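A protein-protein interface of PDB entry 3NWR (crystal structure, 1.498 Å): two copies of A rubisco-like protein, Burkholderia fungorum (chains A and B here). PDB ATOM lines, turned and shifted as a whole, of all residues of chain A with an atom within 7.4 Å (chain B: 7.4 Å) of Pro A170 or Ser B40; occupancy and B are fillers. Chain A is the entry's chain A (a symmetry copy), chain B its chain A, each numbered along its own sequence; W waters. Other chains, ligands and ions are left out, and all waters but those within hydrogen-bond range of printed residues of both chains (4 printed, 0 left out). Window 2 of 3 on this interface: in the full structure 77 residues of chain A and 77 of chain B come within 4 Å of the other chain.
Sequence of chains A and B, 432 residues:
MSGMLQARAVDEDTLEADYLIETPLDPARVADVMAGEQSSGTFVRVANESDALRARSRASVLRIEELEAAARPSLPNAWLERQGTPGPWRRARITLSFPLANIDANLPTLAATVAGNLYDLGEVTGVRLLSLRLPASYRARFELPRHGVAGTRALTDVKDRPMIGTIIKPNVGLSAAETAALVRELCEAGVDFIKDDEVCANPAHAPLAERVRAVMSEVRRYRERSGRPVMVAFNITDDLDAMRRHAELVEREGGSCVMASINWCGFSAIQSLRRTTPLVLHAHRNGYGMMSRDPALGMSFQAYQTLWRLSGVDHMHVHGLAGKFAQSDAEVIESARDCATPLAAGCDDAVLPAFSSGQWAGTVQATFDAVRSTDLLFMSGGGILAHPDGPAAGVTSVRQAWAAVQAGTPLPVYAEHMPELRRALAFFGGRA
Pro A170 touches one residue of chain B.
Of the printed residues of chain B, Val A172 touches Ser B39, Ser B40, Ser B57 and Asn B102.
Printed residues of chain A within 4 Å of Gln B38: Val A199 (3.8 Å).
No residue of chain A comes within 4 Å of Gly B41.
Of the printed residues of chain A, Ser B57 touches Val A172 (3.8 Å) and Gly A173 (3.8 Å).
Printed residues of chain A within 4 Å of Asn B102: Val A172 (3.7 Å) and Val A199 (3.97 Å).
Of the 14 printed residues of chain B, 7 touch a printed residue of chain A.
Of the 14 printed residues of chain A, 6 touch a printed residue of chain B.
Pro A170 touches Ser B40 (CB to O, 3.8 Å).
C of Ser B39 touches CG1 of Val A172, at 3.8 Å.
Val A172 touches Ser B40 (O to CB, 3.2 Å).
O of Val A172 touches OG of Ser B57, at 3.8 Å.
Val A172 touches Asn B102 (CG1 to ND2, 3.7 Å).
Gly A173 touches Ser B57.
CG1 of Val A199 touches O of Gln B38, at 3.8 Å.
Asn B102 touches Val A199 (O to O, 3.97 Å).
No position is printed for both chains.
Of the 12 pairs that touch across the chains among the printed residues, none has its exchanged pair printed and touching as well.
The backbone carbonyl oxygen of Ala B35 sits at hydrogen-bond distance from the side-chain hydroxyl of Ser B39 (2.7 Å).
The side-chain hydroxyl (OG) of Ser B39 lies within hydrogen-bond range of the backbone NH (N) of Ala B59 (2.9 Å).
The side-chain hydroxyl (OG) of Ser B40 lies within hydrogen-bond range of the side-chain hydroxyl (OG) of Ser B57, 3.0 Å away.
OG of Ser B40 lies close to N of Arg B58, at 3.4 Å.
O of Ser B57 is in hydrogen-bond range of ND2 of Asn B102 (2.8 Å).
NZ of Lys A169 sits at hydrogen-bond distance from OD1 of Asn A171 (2.7 Å).
Water W3 lies within hydrogen-bond range of the backbone carbonyl oxygen of Asn B102 and the backbone carbonyl oxygen of Val A199.
Water W1 lies within hydrogen-bond range of OE1 of Glu B37, NZ of Lys A169 and ND2 of Asn A171.
Water W2 bridges O of Glu B37 (2.9 Å) and OD2 of Asp A197 (2.9 Å).
Water W4 lies within hydrogen-bond range of N of Asn A171 (2.9 Å), O of Ser B40 (3.3 Å) and N of Gly B41 (3.3 Å).
O of Glu B37 lies within hydrogen-bond range of ND2 of Asn A171 (3.0 Å).
The backbone carbonyl oxygen of Ser B39 lies close to the side-chain amide nitrogen of Asn A171, 3.2 Å away.
NH2 of Arg B56 lies within hydrogen-bond range of O of Gly A173 (2.7 Å).
NH2 of Arg B56 is in salt-bridge range of OE1 of Glu A178, 3.4 Å away.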
ATOM      1  N   ILE A 167      20.018   7.105  -6.750  1.00  0.00           N
ATOM      2  CA  ILE A 167      19.187   6.733  -7.892  1.00  0.00           C
ATOM      3  C   ILE A 167      18.268   7.889  -8.256  1.00  0.00           C
ATOM      4  O   ILE A 167      17.749   8.584  -7.388  1.00  0.00           O
ATOM      5  CB  ILE A 167      18.318   5.469  -7.617  1.00  0.00           C
ATOM      6  CG1 ILE A 167      19.185   4.303  -7.137  1.00  0.00           C
ATOM      7  CG2 ILE A 167      17.538   5.049  -8.870  1.00  0.00           C
ATOM      8  CD1 ILE A 167      19.538   4.360  -5.666  1.00  0.00           C
ATOM      9  N   ILE A 168      18.090   8.100  -9.551  1.00  0.00           N
ATOM     10  CA  ILE A 168      17.185   9.128 -10.044  1.00  0.00           C
ATOM     11  C   ILE A 168      15.730   8.795  -9.694  1.00  0.00           C
ATOM     12  O   ILE A 168      15.223   7.730 -10.050  1.00  0.00           O
ATOM     13  CB  ILE A 168      17.355   9.293 -11.571  1.00  0.00           C
ATOM     14  CG1 ILE A 168      18.736   9.879 -11.880  1.00  0.00           C
ATOM     15  CG2 ILE A 168      16.254  10.191 -12.143  1.00  0.00           C
ATOM     16  CD1 ILE A 168      19.153   9.740 -13.337  1.00  0.00           C
ATOM     17  N   LYS A 169      15.079   9.711  -8.976  1.00  0.00           N
ATOM     18  CA  LYS A 169      13.680   9.581  -8.567  1.00  0.00           C
ATOM     19  C   LYS A 169      12.918  10.818  -9.030  1.00  0.00           C
ATOM     20  O   LYS A 169      13.457  11.924  -8.980  1.00  0.00           O
ATOM     21  CB  LYS A 169      13.588   9.510  -7.040  1.00  0.00           C
ATOM     22  CG  LYS A 169      14.205   8.275  -6.409  1.00  0.00           C
ATOM     23  CD  LYS A 169      13.283   7.080  -6.562  1.00  0.00           C
ATOM     24  CE  LYS A 169      13.867   5.840  -5.921  1.00  0.00           C
ATOM     25  NZ  LYS A 169      12.930   4.691  -6.048  1.00  0.00           N
ATOM     26  N   PRO A 170      11.663  10.651  -9.479  1.00  0.00           N
ATOM     27  CA  PRO A 170      10.904   9.400  -9.616  1.00  0.00           C
ATOM     28  C   PRO A 170      11.571   8.425 -10.578  1.00  0.00           C
ATOM     29  O   PRO A 170      12.335   8.848 -11.453  1.00  0.00           O
ATOM     30  CB  PRO A 170       9.565   9.864 -10.199  1.00  0.00           C
ATOM     31  CG  PRO A 170       9.886  11.143 -10.887  1.00  0.00           C
ATOM     32  CD  PRO A 170      10.906  11.801 -10.004  1.00  0.00           C
ATOM     33  N   ASN A 171      11.270   7.138 -10.414  1.00  0.00           N
ATOM     34  CA  ASN A 171      11.936   6.078 -11.175  1.00  0.00           C
ATOM     35  C   ASN A 171      11.836   6.300 -12.668  1.00  0.00           C
ATOM     36  O   ASN A 171      12.777   6.041 -13.416  1.00  0.00           O
ATOM     37  CB  ASN A 171      11.320   4.713 -10.853  1.00  0.00           C
ATOM     38  CG  ASN A 171      11.500   4.307  -9.404  1.00  0.00           C
ATOM     39  OD1 ASN A 171      12.418   4.762  -8.724  1.00  0.00           O
ATOM     40  ND2 ASN A 171      10.622   3.426  -8.929  1.00  0.00           N
ATOM     41  N   VAL A 172      10.663   6.747 -13.096  1.00  0.00           N
ATOM     42  CA  VAL A 172      10.399   6.992 -14.505  1.00  0.00           C
ATOM     43  C   VAL A 172       9.312   8.061 -14.576  1.00  0.00           C
ATOM     44  O   VAL A 172       8.481   8.160 -13.674  1.00  0.00           O
ATOM     45  CB  VAL A 172       9.977   5.681 -15.237  1.00  0.00           C
ATOM     46  CG1 VAL A 172       8.629   5.133 -14.706  1.00  0.00           C
ATOM     47  CG2 VAL A 172       9.938   5.895 -16.741  1.00  0.00           C
ATOM     48  N   GLY A 173       9.333   8.883 -15.617  1.00  0.00           N
ATOM     49  CA  GLY A 173       8.294   9.889 -15.780  1.00  0.00           C
ATOM     50  C   GLY A 173       8.799  11.306 -15.970  1.00  0.00           C
ATOM     51  O   GLY A 173       8.099  12.142 -16.546  1.00  0.00           O
ATOM     52  N   LEU A 174       9.995  11.598 -15.466  1.00  0.00           N
ATOM     53  CA  LEU A 174      10.625  12.886 -15.740  1.00  0.00           C
ATOM     54  C   LEU A 174      10.958  13.024 -17.214  1.00  0.00           C
ATOM     55  O   LEU A 174      11.259  12.045 -17.898  1.00  0.00           O
ATOM     56  CB  LEU A 174      11.912  13.060 -14.934  1.00  0.00           C
ATOM     57  CG  LEU A 174      11.832  13.079 -13.407  1.00  0.00           C
ATOM     58  CD1 LEU A 174      13.227  13.230 -12.826  1.00  0.00           C
ATOM     59  CD2 LEU A 174      10.922  14.198 -12.912  1.00  0.00           C
ATOM     60  N   GLU A 178      14.105  17.547 -17.251  1.00  0.00           N
ATOM     61  CA  GLU A 178      13.895  17.430 -15.812  1.00  0.00           C
ATOM     62  C   GLU A 178      14.926  16.487 -15.191  1.00  0.00           C
ATOM     63  O   GLU A 178      15.427  16.730 -14.093  1.00  0.00           O
ATOM     64  CB  GLU A 178      12.473  16.961 -15.506  1.00  0.00           C
ATOM     65  CG  GLU A 178      11.401  18.019 -15.764  1.00  0.00           C
ATOM     66  CD  GLU A 178       9.992  17.463 -15.676  1.00  0.00           C
ATOM     67  OE1 GLU A 178       9.803  16.259 -15.938  1.00  0.00           O
ATOM     68  OE2 GLU A 178       9.065  18.237 -15.355  1.00  0.00           O
ATOM     69  N   THR A 179      15.252  15.416 -15.910  1.00  0.00           N
ATOM     70  CA  THR A 179      16.237  14.459 -15.414  1.00  0.00           C
ATOM     71  C   THR A 179      17.604  15.122 -15.304  1.00  0.00           C
ATOM     72  O   THR A 179      18.306  14.982 -14.298  1.00  0.00           O
ATOM     73  CB  THR A 179      16.339  13.249 -16.346  1.00  0.00           C
ATOM     74  OG1 THR A 179      15.049  12.641 -16.476  1.00  0.00           O
ATOM     75  CG2 THR A 179      17.324  12.208 -15.785  1.00  0.00           C
ATOM     76  N   LEU A 182      17.797  17.483 -12.391  1.00  0.00           N
ATOM     77  CA  LEU A 182      17.910  16.733 -11.150  1.00  0.00           C
ATOM     78  C   LEU A 182      19.321  16.193 -10.986  1.00  0.00           C
ATOM     79  O   LEU A 182      19.917  16.292  -9.916  1.00  0.00           O
ATOM     80  CB  LEU A 182      16.900  15.588 -11.128  1.00  0.00           C
ATOM     81  CG  LEU A 182      17.046  14.588  -9.983  1.00  0.00           C
ATOM     82  CD1 LEU A 182      17.022  15.275  -8.622  1.00  0.00           C
ATOM     83  CD2 LEU A 182      15.952  13.544 -10.097  1.00  0.00           C
ATOM     84  N   ASP A 197      16.819   4.233 -12.532  1.00  0.00           N
ATOM     85  CA  ASP A 197      16.101   3.076 -12.022  1.00  0.00           C
ATOM     86  C   ASP A 197      15.920   2.030 -13.130  1.00  0.00           C
ATOM     87  O   ASP A 197      15.869   2.367 -14.309  1.00  0.00           O
ATOM     88  CB  ASP A 197      14.736   3.485 -11.473  1.00  0.00           C
ATOM     89  CG  ASP A 197      14.064   2.355 -10.724  1.00  0.00           C
ATOM     90  OD1 ASP A 197      14.449   2.111  -9.556  1.00  0.00           O
ATOM     91  OD2 ASP A 197      13.186   1.684 -11.312  1.00  0.00           O
ATOM     92  N   VAL A 199      13.379   0.467 -14.129  1.00  0.00           N
ATOM     93  CA  VAL A 199      12.175   0.584 -14.950  1.00  0.00           C
ATOM     94  C   VAL A 199      12.261   1.738 -15.950  1.00  0.00           C
ATOM     95  O   VAL A 199      11.355   1.916 -16.746  1.00  0.00           O
ATOM     96  CB  VAL A 199      10.871   0.658 -14.110  1.00  0.00           C
ATOM     97  CG1 VAL A 199      10.807  -0.526 -13.136  1.00  0.00           C
ATOM     98  CG2 VAL A 199      10.765   2.004 -13.370  1.00  0.00           C
ATOM     99  N   CYS A 200      13.356   2.496 -15.916  1.00  0.00           N
ATOM    100  CA  CYS A 200      13.573   3.585 -16.864  1.00  0.00           C
ATOM    101  C   CYS A 200      14.728   3.254 -17.791  1.00  0.00           C
ATOM    102  O   CYS A 200      15.879   3.243 -17.365  1.00  0.00           O
ATOM    103  CB  CYS A 200      13.897   4.877 -16.117  1.00  0.00           C
ATOM    104  SG  CYS A 200      14.080   6.288 -17.228  1.00  0.00           S
ATOM    105  N   ALA B  35       2.621  -1.171  -7.436  1.00  0.00           N
ATOM    106  CA  ALA B  35       2.335  -0.267  -8.543  1.00  0.00           C
ATOM    107  C   ALA B  35       3.298   0.916  -8.550  1.00  0.00           C
ATOM    108  O   ALA B  35       3.825   1.303  -9.601  1.00  0.00           O
ATOM    109  CB  ALA B  35       0.890   0.223  -8.461  1.00  0.00           C
ATOM    110  N   GLY B  36       3.532   1.487  -7.374  1.00  0.00           N
ATOM    111  CA  GLY B  36       4.395   2.648  -7.257  1.00  0.00           C
ATOM    112  C   GLY B  36       5.843   2.315  -7.541  1.00  0.00           C
ATOM    113  O   GLY B  36       6.524   3.031  -8.281  1.00  0.00           O
ATOM    114  N   GLU B  37       6.318   1.224  -6.951  1.00  0.00           N
ATOM    115  CA  GLU B  37       7.718   0.846  -7.103  1.00  0.00           C
ATOM    116  C   GLU B  37       8.081   0.528  -8.546  1.00  0.00           C
ATOM    117  O   GLU B  37       9.203   0.795  -8.975  1.00  0.00           O
ATOM    118  CB  GLU B  37       8.056  -0.337  -6.198  1.00  0.00           C
ATOM    119  CG  GLU B  37       8.123   0.052  -4.738  1.00  0.00           C
ATOM    120  CD  GLU B  37       9.199   1.089  -4.490  1.00  0.00           C
ATOM    121  OE1 GLU B  37      10.389   0.750  -4.676  1.00  0.00           O
ATOM    122  OE2 GLU B  37       8.856   2.238  -4.135  1.00  0.00           O
ATOM    123  N   GLN B  38       7.129  -0.024  -9.293  1.00  0.00           N
ATOM    124  CA  GLN B  38       7.379  -0.420 -10.679  1.00  0.00           C
ATOM    125  C   GLN B  38       7.062   0.700 -11.664  1.00  0.00           C
ATOM    126  O   GLN B  38       7.109   0.501 -12.879  1.00  0.00           O
ATOM    127  CB  GLN B  38       6.584  -1.674 -11.036  1.00  0.00           C
ATOM    128  CG  GLN B  38       6.949  -2.901 -10.199  1.00  0.00           C
ATOM    129  CD  GLN B  38       8.447  -3.150 -10.131  1.00  0.00           C
ATOM    130  OE1 GLN B  38       9.080  -2.923  -9.095  1.00  0.00           O
ATOM    131  NE2 GLN B  38       9.021  -3.619 -11.232  1.00  0.00           N
ATOM    132  N   SER B  39       6.745   1.874 -11.136  1.00  0.00           N
ATOM    133  CA  SER B  39       6.525   3.042 -11.974  1.00  0.00           C
ATOM    134  C   SER B  39       7.109   4.287 -11.314  1.00  0.00           C
ATOM    135  O   SER B  39       8.293   4.301 -10.981  1.00  0.00           O
ATOM    136  CB  SER B  39       5.045   3.203 -12.348  1.00  0.00           C
ATOM    137  OG  SER B  39       4.231   3.445 -11.214  1.00  0.00           O
ATOM    138  N   SER B  40       6.294   5.314 -11.101  1.00  0.00           N
ATOM    139  CA  SER B  40       6.811   6.602 -10.615  1.00  0.00           C
ATOM    140  C   SER B  40       6.571   6.898  -9.126  1.00  0.00           C
ATOM    141  O   SER B  40       6.618   8.060  -8.705  1.00  0.00           O
ATOM    142  CB  SER B  40       6.218   7.737 -11.437  1.00  0.00           C
ATOM    143  OG  SER B  40       4.805   7.700 -11.373  1.00  0.00           O
ATOM    144  N   GLY B  41       6.314   5.860  -8.338  1.00  0.00           N
ATOM    145  CA  GLY B  41       6.136   6.016  -6.903  1.00  0.00           C
ATOM    146  C   GLY B  41       4.945   6.888  -6.552  1.00  0.00           C
ATOM    147  O   GLY B  41       5.111   7.986  -6.011  1.00  0.00           O
ATOM    148  N   ALA B  55       0.258  11.504 -13.596  1.00  0.00           N
ATOM    149  CA  ALA B  55      -0.870  11.144 -14.445  1.00  0.00           C
ATOM    150  C   ALA B  55      -0.411  10.342 -15.662  1.00  0.00           C
ATOM    151  O   ALA B  55      -1.134   9.478 -16.163  1.00  0.00           O
ATOM    152  CB  ALA B  55      -1.618  12.398 -14.886  1.00  0.00           C
ATOM    153  N   ARG B  56       0.799  10.628 -16.128  1.00  0.00           N
ATOM    154  CA  ARG B  56       1.314  10.009 -17.344  1.00  0.00           C
ATOM    155  C   ARG B  56       2.179   8.788 -17.038  1.00  0.00           C
ATOM    156  O   ARG B  56       2.544   8.041 -17.947  1.00  0.00           O
ATOM    157  CB  ARG B  56       2.148  11.022 -18.128  1.00  0.00           C
ATOM    158  CG  ARG B  56       3.444  11.420 -17.422  1.00  0.00           C
ATOM    159  CD  ARG B  56       4.170  12.546 -18.140  1.00  0.00           C
ATOM    160  NE  ARG B  56       5.343  12.995 -17.395  1.00  0.00           N
ATOM    161  CZ  ARG B  56       5.900  14.197 -17.527  1.00  0.00           C
ATOM    162  NH1 ARG B  56       5.389  15.075 -18.381  1.00  0.00           N
ATOM    163  NH2 ARG B  56       6.965  14.526 -16.800  1.00  0.00           N
ATOM    164  N   SER B  57       2.509   8.593 -15.764  1.00  0.00           N
ATOM    165  CA  SER B  57       3.553   7.631 -15.412  1.00  0.00           C
ATOM    166  C   SER B  57       3.262   6.717 -14.228  1.00  0.00           C
ATOM    167  O   SER B  57       3.997   5.762 -14.000  1.00  0.00           O
ATOM    168  CB  SER B  57       4.867   8.363 -15.146  1.00  0.00           C
ATOM    169  OG  SER B  57       4.776   9.153 -13.968  1.00  0.00           O
ATOM    170  N   ARG B  58       2.224   7.001 -13.454  1.00  0.00           N
ATOM    171  CA  ARG B  58       1.968   6.185 -12.272  1.00  0.00           C
ATOM    172  C   ARG B  58       1.061   5.002 -12.611  1.00  0.00           C
ATOM    173  O   ARG B  58      -0.049   5.184 -13.125  1.00  0.00           O
ATOM    174  CB  ARG B  58       1.378   7.048 -11.142  1.00  0.00           C
ATOM    175  CG  ARG B  58       1.007   6.303  -9.858  1.00  0.00           C
ATOM    176  CD  ARG B  58       2.202   5.574  -9.263  1.00  0.00           C
ATOM    177  NE  ARG B  58       2.146   5.498  -7.801  1.00  0.00           N
ATOM    178  CZ  ARG B  58       1.388   4.650  -7.111  1.00  0.00           C
ATOM    179  NH1 ARG B  58       0.598   3.782  -7.738  1.00  0.00           N
ATOM    180  NH2 ARG B  58       1.423   4.668  -5.784  1.00  0.00           N
ATOM    181  N   ALA B  59       1.552   3.788 -12.364  1.00  0.00           N
ATOM    182  CA  ALA B  59       0.732   2.587 -12.526  1.00  0.00           C
ATOM    183  C   ALA B  59      -0.365   2.575 -11.465  1.00  0.00           C
ATOM    184  O   ALA B  59      -0.224   3.192 -10.411  1.00  0.00           O
ATOM    185  CB  ALA B  59       1.590   1.330 -12.419  1.00  0.00           C
ATOM    186  N   PRO B  99       1.181   2.356 -17.646  1.00  0.00           N
ATOM    187  CA  PRO B  99       1.198   3.217 -18.833  1.00  0.00           C
ATOM    188  C   PRO B  99       2.301   2.813 -19.809  1.00  0.00           C
ATOM    189  O   PRO B  99       3.473   2.738 -19.431  1.00  0.00           O
ATOM    190  CB  PRO B  99       1.495   4.615 -18.264  1.00  0.00           C
ATOM    191  CG  PRO B  99       1.308   4.508 -16.792  1.00  0.00           C
ATOM    192  CD  PRO B  99       1.586   3.079 -16.431  1.00  0.00           C
ATOM    193  N   ASN B 102       5.718   4.616 -20.263  1.00  0.00           N
ATOM    194  CA  ASN B 102       6.837   4.349 -19.356  1.00  0.00           C
ATOM    195  C   ASN B 102       7.861   3.400 -19.972  1.00  0.00           C
ATOM    196  O   ASN B 102       9.041   3.424 -19.599  1.00  0.00           O
ATOM    197  CB  ASN B 102       6.350   3.715 -18.048  1.00  0.00           C
ATOM    198  CG  ASN B 102       5.646   4.693 -17.137  1.00  0.00           C
ATOM    199  OD1 ASN B 102       5.421   5.845 -17.495  1.00  0.00           O
ATOM    200  ND2 ASN B 102       5.293   4.233 -15.939  1.00  0.00           N
HETATM  201  O   HOH W   1      11.939   1.832  -6.629  1.00  0.00           O
HETATM  202  O   HOH W   2      11.994   0.198  -9.155  1.00  0.00           O
HETATM  203  O   HOH W   3      11.521   2.504 -19.404  1.00  0.00           O
HETATM  204  O   HOH W   4       9.516   6.616  -8.211  1.00  0.00           O
